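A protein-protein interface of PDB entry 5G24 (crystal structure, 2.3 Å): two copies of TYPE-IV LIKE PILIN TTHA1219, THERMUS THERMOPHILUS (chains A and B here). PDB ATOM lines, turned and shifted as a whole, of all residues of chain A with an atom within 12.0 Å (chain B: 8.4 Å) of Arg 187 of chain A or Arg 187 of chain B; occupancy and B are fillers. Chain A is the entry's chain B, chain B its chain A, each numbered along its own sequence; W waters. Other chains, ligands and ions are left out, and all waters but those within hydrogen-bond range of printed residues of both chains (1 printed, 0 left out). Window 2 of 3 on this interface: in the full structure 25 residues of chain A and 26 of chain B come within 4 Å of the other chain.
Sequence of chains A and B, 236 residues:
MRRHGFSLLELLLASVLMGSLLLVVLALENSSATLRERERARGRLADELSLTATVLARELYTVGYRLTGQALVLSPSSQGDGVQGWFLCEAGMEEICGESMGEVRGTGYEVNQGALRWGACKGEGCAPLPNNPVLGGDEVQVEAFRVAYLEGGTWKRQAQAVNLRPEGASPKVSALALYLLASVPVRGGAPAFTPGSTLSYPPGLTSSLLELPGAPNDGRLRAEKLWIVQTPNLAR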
ATOM      1  N   GLU A  39      -9.827 -11.666  13.490  1.00  0.00           N
ATOM      2  CA  GLU A  39     -10.531 -12.684  14.367  1.00  0.00           C
ATOM      3  C   GLU A  39     -11.826 -11.949  14.899  1.00  0.00           C
ATOM      4  O   GLU A  39     -12.219 -10.804  14.441  1.00  0.00           O
ATOM      5  CB  GLU A  39      -9.509 -13.216  15.466  1.00  0.00           C
ATOM      6  CG  GLU A  39      -9.855 -14.309  16.524  1.00  0.00           C
ATOM      7  CD  GLU A  39     -10.385 -15.643  15.990  1.00  0.00           C
ATOM      8  OE1 GLU A  39     -11.417 -15.644  15.274  1.00  0.00           O
ATOM      9  OE2 GLU A  39      -9.814 -16.711  16.342  1.00  0.00           O
ATOM     10  N   ARG A  40     -12.521 -12.659  15.775  1.00  0.00           N
ATOM     11  CA  ARG A  40     -13.430 -12.087  16.775  1.00  0.00           C
ATOM     12  C   ARG A  40     -12.741 -10.954  17.533  1.00  0.00           C
ATOM     13  O   ARG A  40     -13.305  -9.929  17.748  1.00  0.00           O
ATOM     14  CB  ARG A  40     -13.869 -13.170  17.761  1.00  0.00           C
ATOM     15  CG  ARG A  40     -15.076 -13.982  17.295  1.00  0.00           C
ATOM     16  CD  ARG A  40     -15.545 -15.045  18.306  1.00  0.00           C
ATOM     17  NE  ARG A  40     -14.388 -15.707  18.937  1.00  0.00           N
ATOM     18  CZ  ARG A  40     -13.973 -15.556  20.209  1.00  0.00           C
ATOM     19  NH1 ARG A  40     -14.617 -14.765  21.080  1.00  0.00           N
ATOM     20  NH2 ARG A  40     -12.896 -16.228  20.631  1.00  0.00           N
ATOM     21  N   ALA A  41     -11.494 -11.193  17.922  1.00  0.00           N
ATOM     22  CA  ALA A  41     -10.696 -10.278  18.716  1.00  0.00           C
ATOM     23  C   ALA A  41     -10.595  -8.910  18.028  1.00  0.00           C
ATOM     24  O   ALA A  41     -10.751  -7.926  18.685  1.00  0.00           O
ATOM     25  CB  ALA A  41      -9.318 -10.871  19.016  1.00  0.00           C
ATOM     26  N   ARG A  42     -10.290  -8.921  16.722  1.00  0.00           N
ATOM     27  CA  ARG A  42     -10.084  -7.699  15.885  1.00  0.00           C
ATOM     28  C   ARG A  42     -11.371  -6.883  15.700  1.00  0.00           C
ATOM     29  O   ARG A  42     -11.390  -5.689  15.891  1.00  0.00           O
ATOM     30  CB  ARG A  42      -9.482  -8.103  14.532  1.00  0.00           C
ATOM     31  CG  ARG A  42      -9.880  -7.293  13.299  1.00  0.00           C
ATOM     32  CD  ARG A  42     -10.959  -8.078  12.528  1.00  0.00           C
ATOM     33  NE  ARG A  42     -11.377  -7.383  11.308  1.00  0.00           N
ATOM     34  CZ  ARG A  42     -10.763  -7.482  10.118  1.00  0.00           C
ATOM     35  NH1 ARG A  42      -9.694  -8.291   9.945  1.00  0.00           N
ATOM     36  NH2 ARG A  42     -11.222  -6.767   9.078  1.00  0.00           N
ATOM     37  N   ARG A  44     -13.911  -6.938  17.866  1.00  0.00           N
ATOM     38  CA  ARG A  44     -14.183  -6.359  19.147  1.00  0.00           C
ATOM     39  C   ARG A  44     -13.293  -5.117  19.429  1.00  0.00           C
ATOM     40  O   ARG A  44     -13.799  -4.132  19.960  1.00  0.00           O
ATOM     41  CB  ARG A  44     -14.015  -7.351  20.242  1.00  0.00           C
ATOM     42  CG  ARG A  44     -14.175  -6.797  21.634  1.00  0.00           C
ATOM     43  CD  ARG A  44     -13.981  -7.854  22.675  1.00  0.00           C
ATOM     44  NE  ARG A  44     -14.105  -7.285  23.984  1.00  0.00           N
ATOM     45  CZ  ARG A  44     -13.792  -7.887  25.103  1.00  0.00           C
ATOM     46  NH1 ARG A  44     -13.392  -9.142  25.090  1.00  0.00           N
ATOM     47  NH2 ARG A  44     -13.948  -7.277  26.275  1.00  0.00           N
ATOM     48  N   GLU A 139      -5.840  -5.090  29.891  1.00  0.00           N
ATOM     49  CA  GLU A 139      -5.895  -6.047  28.784  1.00  0.00           C
ATOM     50  C   GLU A 139      -5.667  -5.335  27.441  1.00  0.00           C
ATOM     51  O   GLU A 139      -4.933  -5.790  26.573  1.00  0.00           O
ATOM     52  CB  GLU A 139      -7.239  -6.760  28.770  1.00  0.00           C
ATOM     53  CG  GLU A 139      -7.329  -7.811  27.678  1.00  0.00           C
ATOM     54  CD  GLU A 139      -8.410  -8.867  27.882  1.00  0.00           C
ATOM     55  OE1 GLU A 139      -8.537  -9.333  29.001  1.00  0.00           O
ATOM     56  OE2 GLU A 139      -9.175  -9.134  26.936  1.00  0.00           O
ATOM     57  N   SER A 183      -3.530  -2.640  21.284  1.00  0.00           N
ATOM     58  CA  SER A 183      -3.267  -4.073  21.193  1.00  0.00           C
ATOM     59  C   SER A 183      -3.940  -4.874  22.306  1.00  0.00           C
ATOM     60  O   SER A 183      -4.155  -4.331  23.396  1.00  0.00           O
ATOM     61  CB  SER A 183      -1.755  -4.335  21.210  1.00  0.00           C
ATOM     62  OG  SER A 183      -1.203  -4.045  22.501  1.00  0.00           O
ATOM     63  N   VAL A 184      -4.279  -6.133  21.983  1.00  0.00           N
ATOM     64  CA  VAL A 184      -4.749  -7.078  22.946  1.00  0.00           C
ATOM     65  C   VAL A 184      -4.027  -8.405  22.800  1.00  0.00           C
ATOM     66  O   VAL A 184      -3.588  -8.731  21.704  1.00  0.00           O
ATOM     67  CB  VAL A 184      -6.292  -7.327  22.838  1.00  0.00           C
ATOM     68  CG1 VAL A 184      -7.030  -6.059  23.142  1.00  0.00           C
ATOM     69  CG2 VAL A 184      -6.721  -7.816  21.458  1.00  0.00           C
ATOM     70  N   PRO A 185      -3.938  -9.203  23.903  1.00  0.00           N
ATOM     71  CA  PRO A 185      -3.427 -10.560  23.817  1.00  0.00           C
ATOM     72  C   PRO A 185      -4.373 -11.470  23.114  1.00  0.00           C
ATOM     73  O   PRO A 185      -5.569 -11.271  23.176  1.00  0.00           O
ATOM     74  CB  PRO A 185      -3.320 -11.006  25.273  1.00  0.00           C
ATOM     75  CG  PRO A 185      -4.379 -10.221  25.944  1.00  0.00           C
ATOM     76  CD  PRO A 185      -4.518  -8.936  25.237  1.00  0.00           C
ATOM     77  N   VAL A 186      -3.849 -12.392  22.370  1.00  0.00           N
ATOM     78  CA  VAL A 186      -4.723 -13.359  21.682  1.00  0.00           C
ATOM     79  C   VAL A 186      -4.088 -14.761  21.778  1.00  0.00           C
ATOM     80  O   VAL A 186      -2.877 -14.888  21.754  1.00  0.00           O
ATOM     81  CB  VAL A 186      -5.010 -12.946  20.245  1.00  0.00           C
ATOM     82  CG1 VAL A 186      -6.001 -13.868  19.599  1.00  0.00           C
ATOM     83  CG2 VAL A 186      -5.600 -11.544  20.201  1.00  0.00           C
ATOM     84  N   ARG A 187      -4.929 -15.772  21.856  1.00  0.00           N
ATOM     85  CA  ARG A 187      -4.481 -17.115  22.101  1.00  0.00           C
ATOM     86  C   ARG A 187      -3.671 -17.621  20.887  1.00  0.00           C
ATOM     87  O   ARG A 187      -4.135 -17.576  19.735  1.00  0.00           O
ATOM     88  CB  ARG A 187      -5.678 -18.025  22.389  1.00  0.00           C
ATOM     89  CG  ARG A 187      -5.328 -19.300  23.146  1.00  0.00           C
ATOM     90  CD  ARG A 187      -6.493 -20.301  23.026  1.00  0.00           C
ATOM     91  NE  ARG A 187      -6.111 -21.664  23.315  1.00  0.00           N
ATOM     92  CZ  ARG A 187      -6.302 -22.311  24.480  1.00  0.00           C
ATOM     93  NH1 ARG A 187      -6.864 -21.699  25.546  1.00  0.00           N
ATOM     94  NH2 ARG A 187      -5.925 -23.597  24.585  1.00  0.00           N
ATOM     95  N   GLY A 188      -2.441 -18.069  21.166  1.00  0.00           N
ATOM     96  CA  GLY A 188      -1.528 -18.516  20.118  1.00  0.00           C
ATOM     97  C   GLY A 188      -0.819 -17.394  19.329  1.00  0.00           C
ATOM     98  O   GLY A 188      -0.043 -17.665  18.418  1.00  0.00           O
ATOM     99  N   GLY A 189      -1.070 -16.155  19.693  1.00  0.00           N
ATOM    100  CA  GLY A 189      -0.398 -15.045  19.069  1.00  0.00           C
ATOM    101  C   GLY A 189      -1.022 -14.678  17.731  1.00  0.00           C
ATOM    102  O   GLY A 189      -1.700 -15.490  17.123  1.00  0.00           O
ATOM    103  N   ALA A 190      -0.797 -13.454  17.310  1.00  0.00           N
ATOM    104  CA  ALA A 190      -1.237 -12.972  16.035  1.00  0.00           C
ATOM    105  C   ALA A 190      -0.065 -12.506  15.125  1.00  0.00           C
ATOM    106  O   ALA A 190       1.031 -12.183  15.606  1.00  0.00           O
ATOM    107  CB  ALA A 190      -2.191 -11.817  16.271  1.00  0.00           C
ATOM    108  N   PRO A 191      -0.300 -12.481  13.796  1.00  0.00           N
ATOM    109  CA  PRO A 191       0.776 -12.105  12.898  1.00  0.00           C
ATOM    110  C   PRO A 191       1.064 -10.616  12.970  1.00  0.00           C
ATOM    111  O   PRO A 191       0.263  -9.845  13.503  1.00  0.00           O
ATOM    112  CB  PRO A 191       0.239 -12.475  11.500  1.00  0.00           C
ATOM    113  CG  PRO A 191      -1.249 -12.433  11.658  1.00  0.00           C
ATOM    114  CD  PRO A 191      -1.487 -12.960  13.047  1.00  0.00           C
ATOM    115  N   ASP A 218       5.355  -9.186  18.928  1.00  0.00           N
ATOM    116  CA  ASP A 218       5.218  -9.715  20.275  1.00  0.00           C
ATOM    117  C   ASP A 218       4.070 -10.726  20.424  1.00  0.00           C
ATOM    118  O   ASP A 218       3.809 -11.198  21.528  1.00  0.00           O
ATOM    119  CB  ASP A 218       5.056  -8.559  21.277  1.00  0.00           C
ATOM    120  CG  ASP A 218       3.786  -7.745  21.064  1.00  0.00           C
ATOM    121  OD1 ASP A 218       3.006  -7.996  20.082  1.00  0.00           O
ATOM    122  OD2 ASP A 218       3.589  -6.814  21.887  1.00  0.00           O
ATOM    123  N   GLY A 219       3.363 -11.040  19.339  1.00  0.00           N
ATOM    124  CA  GLY A 219       2.184 -11.898  19.407  1.00  0.00           C
ATOM    125  C   GLY A 219       0.838 -11.214  19.711  1.00  0.00           C
ATOM    126  O   GLY A 219      -0.201 -11.901  19.671  1.00  0.00           O
ATOM    127  N   ARG A 220       0.845  -9.894  20.011  1.00  0.00           N
ATOM    128  CA  ARG A 220      -0.371  -9.190  20.346  1.00  0.00           C
ATOM    129  C   ARG A 220      -1.120  -8.804  19.102  1.00  0.00           C
ATOM    130  O   ARG A 220      -0.502  -8.537  18.131  1.00  0.00           O
ATOM    131  CB  ARG A 220      -0.131  -7.978  21.248  1.00  0.00           C
ATOM    132  CG  ARG A 220       0.333  -8.327  22.637  1.00  0.00           C
ATOM    133  CD  ARG A 220       0.573  -7.142  23.485  1.00  0.00           C
ATOM    134  NE  ARG A 220      -0.636  -6.413  23.801  1.00  0.00           N
ATOM    135  CZ  ARG A 220      -1.334  -6.549  24.923  1.00  0.00           C
ATOM    136  NH1 ARG A 220      -0.977  -7.419  25.817  1.00  0.00           N
ATOM    137  NH2 ARG A 220      -2.425  -5.812  25.119  1.00  0.00           N
ATOM    138  N   LEU A 221      -2.452  -8.847  19.150  1.00  0.00           N
ATOM    139  CA  LEU A 221      -3.289  -8.439  18.038  1.00  0.00           C
ATOM    140  C   LEU A 221      -3.578  -6.945  18.149  1.00  0.00           C
ATOM    141  O   LEU A 221      -3.925  -6.490  19.203  1.00  0.00           O
ATOM    142  CB  LEU A 221      -4.616  -9.177  18.015  1.00  0.00           C
ATOM    143  CG  LEU A 221      -5.484  -8.790  16.793  1.00  0.00           C
ATOM    144  CD1 LEU A 221      -5.973  -9.969  15.985  1.00  0.00           C
ATOM    145  CD2 LEU A 221      -6.661  -7.953  17.216  1.00  0.00           C
ATOM    146  N   ARG A 222      -3.349  -6.252  17.033  1.00  0.00           N
ATOM    147  CA  ARG A 222      -3.387  -4.789  16.919  1.00  0.00           C
ATOM    148  C   ARG A 222      -4.493  -4.292  15.989  1.00  0.00           C
ATOM    149  O   ARG A 222      -4.805  -4.875  14.974  1.00  0.00           O
ATOM    150  CB  ARG A 222      -2.059  -4.214  16.465  1.00  0.00           C
ATOM    151  CG  ARG A 222      -1.058  -4.123  17.623  1.00  0.00           C
ATOM    152  CD  ARG A 222       0.375  -3.773  17.321  1.00  0.00           C
ATOM    153  NE  ARG A 222       1.075  -3.773  18.610  1.00  0.00           N
ATOM    154  CZ  ARG A 222       1.629  -4.830  19.215  1.00  0.00           C
ATOM    155  NH1 ARG A 222       1.626  -6.023  18.676  1.00  0.00           N
ATOM    156  NH2 ARG A 222       2.213  -4.677  20.404  1.00  0.00           N
ATOM    157  N   ALA B  33     -11.007 -20.348  34.821  1.00  0.00           N
ATOM    158  CA  ALA B  33     -10.280 -19.054  34.637  1.00  0.00           C
ATOM    159  C   ALA B  33      -9.638 -18.626  35.950  1.00  0.00           C
ATOM    160  O   ALA B  33     -10.324 -18.630  36.943  1.00  0.00           O
ATOM    161  CB  ALA B  33     -11.245 -17.994  34.177  1.00  0.00           C
ATOM    162  N   THR B  34      -8.370 -18.209  35.936  1.00  0.00           N
ATOM    163  CA  THR B  34      -7.696 -17.663  37.155  1.00  0.00           C
ATOM    164  C   THR B  34      -8.347 -16.375  37.603  1.00  0.00           C
ATOM    165  O   THR B  34      -9.157 -15.821  36.862  1.00  0.00           O
ATOM    166  CB  THR B  34      -6.152 -17.479  37.016  1.00  0.00           C
ATOM    167  OG1 THR B  34      -5.640 -16.811  38.196  1.00  0.00           O
ATOM    168  CG2 THR B  34      -5.784 -16.695  35.802  1.00  0.00           C
ATOM    169  N   GLU B  37      -7.307 -13.495  35.242  1.00  0.00           N
ATOM    170  CA  GLU B  37      -7.838 -13.467  33.901  1.00  0.00           C
ATOM    171  C   GLU B  37      -9.184 -12.864  33.994  1.00  0.00           C
ATOM    172  O   GLU B  37      -9.534 -12.121  33.133  1.00  0.00           O
ATOM    173  CB  GLU B  37      -7.892 -14.837  33.246  1.00  0.00           C
ATOM    174  CG  GLU B  37      -6.528 -15.358  32.763  1.00  0.00           C
ATOM    175  CD  GLU B  37      -6.459 -16.913  32.521  1.00  0.00           C
ATOM    176  OE1 GLU B  37      -7.218 -17.692  33.174  1.00  0.00           O
ATOM    177  OE2 GLU B  37      -5.612 -17.343  31.680  1.00  0.00           O
ATOM    178  N   ARG B  38      -9.939 -13.218  35.032  1.00  0.00           N
ATOM    179  CA  ARG B  38     -11.255 -12.708  35.245  1.00  0.00           C
ATOM    180  C   ARG B  38     -11.280 -11.215  35.534  1.00  0.00           C
ATOM    181  O   ARG B  38     -12.234 -10.519  35.132  1.00  0.00           O
ATOM    182  CB  ARG B  38     -11.991 -13.480  36.354  1.00  0.00           C
ATOM    183  CG  ARG B  38     -12.375 -14.885  35.883  1.00  0.00           C
ATOM    184  CD  ARG B  38     -12.479 -15.877  37.010  1.00  0.00           C
ATOM    185  NE  ARG B  38     -13.202 -15.316  38.143  1.00  0.00           N
ATOM    186  CZ  ARG B  38     -13.052 -15.687  39.416  1.00  0.00           C
ATOM    187  NH1 ARG B  38     -12.203 -16.623  39.725  1.00  0.00           N
ATOM    188  NH2 ARG B  38     -13.755 -15.094  40.368  1.00  0.00           N
ATOM    189  N   ALA B  41     -10.493  -9.415  32.209  1.00  0.00           N
ATOM    190  CA  ALA B  41     -11.638  -9.499  31.338  1.00  0.00           C
ATOM    191  C   ALA B  41     -12.738  -8.591  31.810  1.00  0.00           C
ATOM    192  O   ALA B  41     -13.334  -7.878  30.983  1.00  0.00           O
ATOM    193  CB  ALA B  41     -12.110 -10.933  31.247  1.00  0.00           C
ATOM    194  N   VAL B 184     -18.735 -11.785  28.077  1.00  0.00           N
ATOM    195  CA  VAL B 184     -17.676 -12.266  27.231  1.00  0.00           C
ATOM    196  C   VAL B 184     -17.203 -13.647  27.601  1.00  0.00           C
ATOM    197  O   VAL B 184     -17.322 -14.049  28.728  1.00  0.00           O
ATOM    198  CB  VAL B 184     -16.415 -11.282  27.253  1.00  0.00           C
ATOM    199  CG1 VAL B 184     -16.840  -9.936  26.720  1.00  0.00           C
ATOM    200  CG2 VAL B 184     -15.856 -11.087  28.633  1.00  0.00           C
ATOM    201  N   PRO B 185     -16.578 -14.332  26.637  1.00  0.00           N
ATOM    202  CA  PRO B 185     -15.991 -15.612  26.961  1.00  0.00           C
ATOM    203  C   PRO B 185     -14.720 -15.402  27.713  1.00  0.00           C
ATOM    204  O   PRO B 185     -14.049 -14.431  27.525  1.00  0.00           O
ATOM    205  CB  PRO B 185     -15.655 -16.204  25.560  1.00  0.00           C
ATOM    206  CG  PRO B 185     -15.426 -15.011  24.718  1.00  0.00           C
ATOM    207  CD  PRO B 185     -16.329 -13.967  25.222  1.00  0.00           C
ATOM    208  N   VAL B 186     -14.382 -16.318  28.558  1.00  0.00           N
ATOM    209  CA  VAL B 186     -13.142 -16.262  29.272  1.00  0.00           C
ATOM    210  C   VAL B 186     -12.621 -17.670  29.347  1.00  0.00           C
ATOM    211  O   VAL B 186     -13.389 -18.683  29.439  1.00  0.00           O
ATOM    212  CB  VAL B 186     -13.322 -15.521  30.609  1.00  0.00           C
ATOM    213  CG1 VAL B 186     -14.260 -16.269  31.535  1.00  0.00           C
ATOM    214  CG2 VAL B 186     -11.995 -15.313  31.313  1.00  0.00           C
ATOM    215  N   ARG B 187     -11.302 -17.771  29.286  1.00  0.00           N
ATOM    216  CA  ARG B 187     -10.631 -19.092  29.172  1.00  0.00           C
ATOM    217  C   ARG B 187     -10.826 -19.926  30.458  1.00  0.00           C
ATOM    218  O   ARG B 187     -10.526 -19.510  31.554  1.00  0.00           O
ATOM    219  CB  ARG B 187      -9.160 -18.888  28.859  1.00  0.00           C
ATOM    220  CG  ARG B 187      -8.519 -20.081  28.149  1.00  0.00           C
ATOM    221  CD  ARG B 187      -6.994 -20.105  28.340  1.00  0.00           C
ATOM    222  NE  ARG B 187      -6.696 -20.111  29.777  1.00  0.00           N
ATOM    223  CZ  ARG B 187      -6.726 -21.189  30.558  1.00  0.00           C
ATOM    224  NH1 ARG B 187      -6.975 -22.398  30.054  1.00  0.00           N
ATOM    225  NH2 ARG B 187      -6.487 -21.056  31.859  1.00  0.00           N
ATOM    226  N   GLY B 188     -11.407 -21.087  30.281  1.00  0.00           N
ATOM    227  CA  GLY B 188     -11.724 -21.989  31.411  1.00  0.00           C
ATOM    228  C   GLY B 188     -12.993 -21.641  32.172  1.00  0.00           C
ATOM    229  O   GLY B 188     -13.364 -22.337  33.141  1.00  0.00           O
ATOM    230  N   GLY B 189     -13.704 -20.590  31.734  1.00  0.00           N
ATOM    231  CA  GLY B 189     -15.015 -20.282  32.301  1.00  0.00           C
ATOM    232  C   GLY B 189     -14.905 -19.403  33.505  1.00  0.00           C
ATOM    233  O   GLY B 189     -13.932 -19.458  34.224  1.00  0.00           O
ATOM    234  N   ALA B 190     -15.867 -18.505  33.657  1.00  0.00           N
ATOM    235  CA  ALA B 190     -16.053 -17.768  34.856  1.00  0.00           C
ATOM    236  C   ALA B 190     -17.253 -18.329  35.641  1.00  0.00           C
ATOM    237  O   ALA B 190     -18.176 -18.955  35.072  1.00  0.00           O
ATOM    238  CB  ALA B 190     -16.252 -16.338  34.510  1.00  0.00           C
ATOM    239  N   GLY B 219     -20.464 -20.232  32.054  1.00  0.00           N
ATOM    240  CA  GLY B 219     -19.025 -20.011  31.929  1.00  0.00           C
ATOM    241  C   GLY B 219     -18.561 -18.661  31.319  1.00  0.00           C
ATOM    242  O   GLY B 219     -17.398 -18.363  31.370  1.00  0.00           O
ATOM    243  N   ARG B 220     -19.501 -17.836  30.826  1.00  0.00           N
ATOM    244  CA  ARG B 220     -19.188 -16.515  30.350  1.00  0.00           C
ATOM    245  C   ARG B 220     -19.050 -15.530  31.498  1.00  0.00           C
ATOM    246  O   ARG B 220     -19.772 -15.611  32.492  1.00  0.00           O
ATOM    247  CB  ARG B 220     -20.226 -15.986  29.367  1.00  0.00           C
ATOM    248  CG  ARG B 220     -20.200 -16.776  28.076  1.00  0.00           C
ATOM    249  CD  ARG B 220     -21.239 -16.263  27.122  1.00  0.00           C
ATOM    250  NE  ARG B 220     -20.940 -14.928  26.592  1.00  0.00           N
ATOM    251  CZ  ARG B 220     -20.268 -14.707  25.489  1.00  0.00           C
ATOM    252  NH1 ARG B 220     -19.804 -15.699  24.769  1.00  0.00           N
ATOM    253  NH2 ARG B 220     -20.091 -13.464  25.070  1.00  0.00           N
ATOM    254  N   LEU B 221     -18.151 -14.555  31.328  1.00  0.00           N
ATOM    255  CA  LEU B 221     -18.002 -13.502  32.337  1.00  0.00           C
ATOM    256  C   LEU B 221     -18.968 -12.389  31.982  1.00  0.00           C
ATOM    257  O   LEU B 221     -18.933 -11.937  30.856  1.00  0.00           O
ATOM    258  CB  LEU B 221     -16.576 -13.018  32.374  1.00  0.00           C
ATOM    259  CG  LEU B 221     -16.350 -11.953  33.478  1.00  0.00           C
ATOM    260  CD1 LEU B 221     -15.174 -12.255  34.381  1.00  0.00           C
ATOM    261  CD2 LEU B 221     -16.139 -10.572  32.854  1.00  0.00           C
HETATM  262  O   HOH W   1     -13.526  -8.672  28.471  1.00  0.00           O
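N of Ala 33 of chain B lies close to O of Arg 187 of chain B (3.4 Å).
The side-chain carboxylate of Glu 37 of chain B is in salt-bridge range of the guanidinium group of Arg 187 of chain B (3.5 Å).
The backbone NH of Leu 221 of chain B sits at hydrogen-bond distance from the backbone carbonyl oxygen of Val 184 of chain B (2.8 Å).
The guanidinium group of Arg 220 of chain A sits at hydrogen-bond distance from the backbone carbonyl oxygen of Glu 139 of chain A, at 2.9 Å.
Among the printed residues, pairs that only touch across the chains: Arg 187 of chain A with Arg 187 of chain B, Arg 40 of chain A with Pro 185 of chain B, Glu 139 of chain A with Ala 41 of chain B and Arg 44 of chain A with Val 184 of chain B.
Of the printed residues of chain B, Arg 187 of chain A touches Arg 187.
Of chain A, only Arg 187 (3.2 Å) comes within 4 Å of Arg 187 of chain B.
No residue of chain B comes within 4 Å of Gly 188 of chain A.
No residue of chain A comes within 4 Å of Ala 33 of chain B.
No residue of chain A comes within 4 Å of Thr 34 of chain B.
No residue of chain A comes within 4 Å of Glu 37 of chain B.
Of the printed residues of chain A, Pro 185 of chain B touches Arg 40.
No residue of chain A comes within 4 Å of Val 186 of chain B.
No residue of chain A comes within 4 Å of Gly 188 of chain B.
No residue of chain A comes within 4 Å of Gly 189 of chain B.
Of the printed residues of chain A, Val 184 of chain B touches Arg 44.
Printed residues of chain B within 4 Å of Arg 44 of chain A: Val 184 (3.9 Å).
Of the printed residues of chain B, Arg 40 of chain A touches Pro 185.
Arg 220 of chain A touches none of the printed residues of chain B.
Of the 20 printed residues of chain A, 4 touch a printed residue of chain B.
Of the 15 printed residues of chain B, 4 touch a printed residue of chain A.
Among the printed residues, 4 pairs touch across the chains.
Arg 187 of chain A touches its own counterpart, Arg 187 of chain B.
Positions printed for both chains: 41, 184, 185, 186, 187, 188, 189, 190, 219, 220 and 221.
Of the 4 pairs that touch across the chains among the printed residues, 1 has its exchanged pair printed and touching as well.
Water W1 bridges NH2 of Arg 44 of chain A (2.6 Å) and O of Ala 41 of chain B (2.6 Å).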
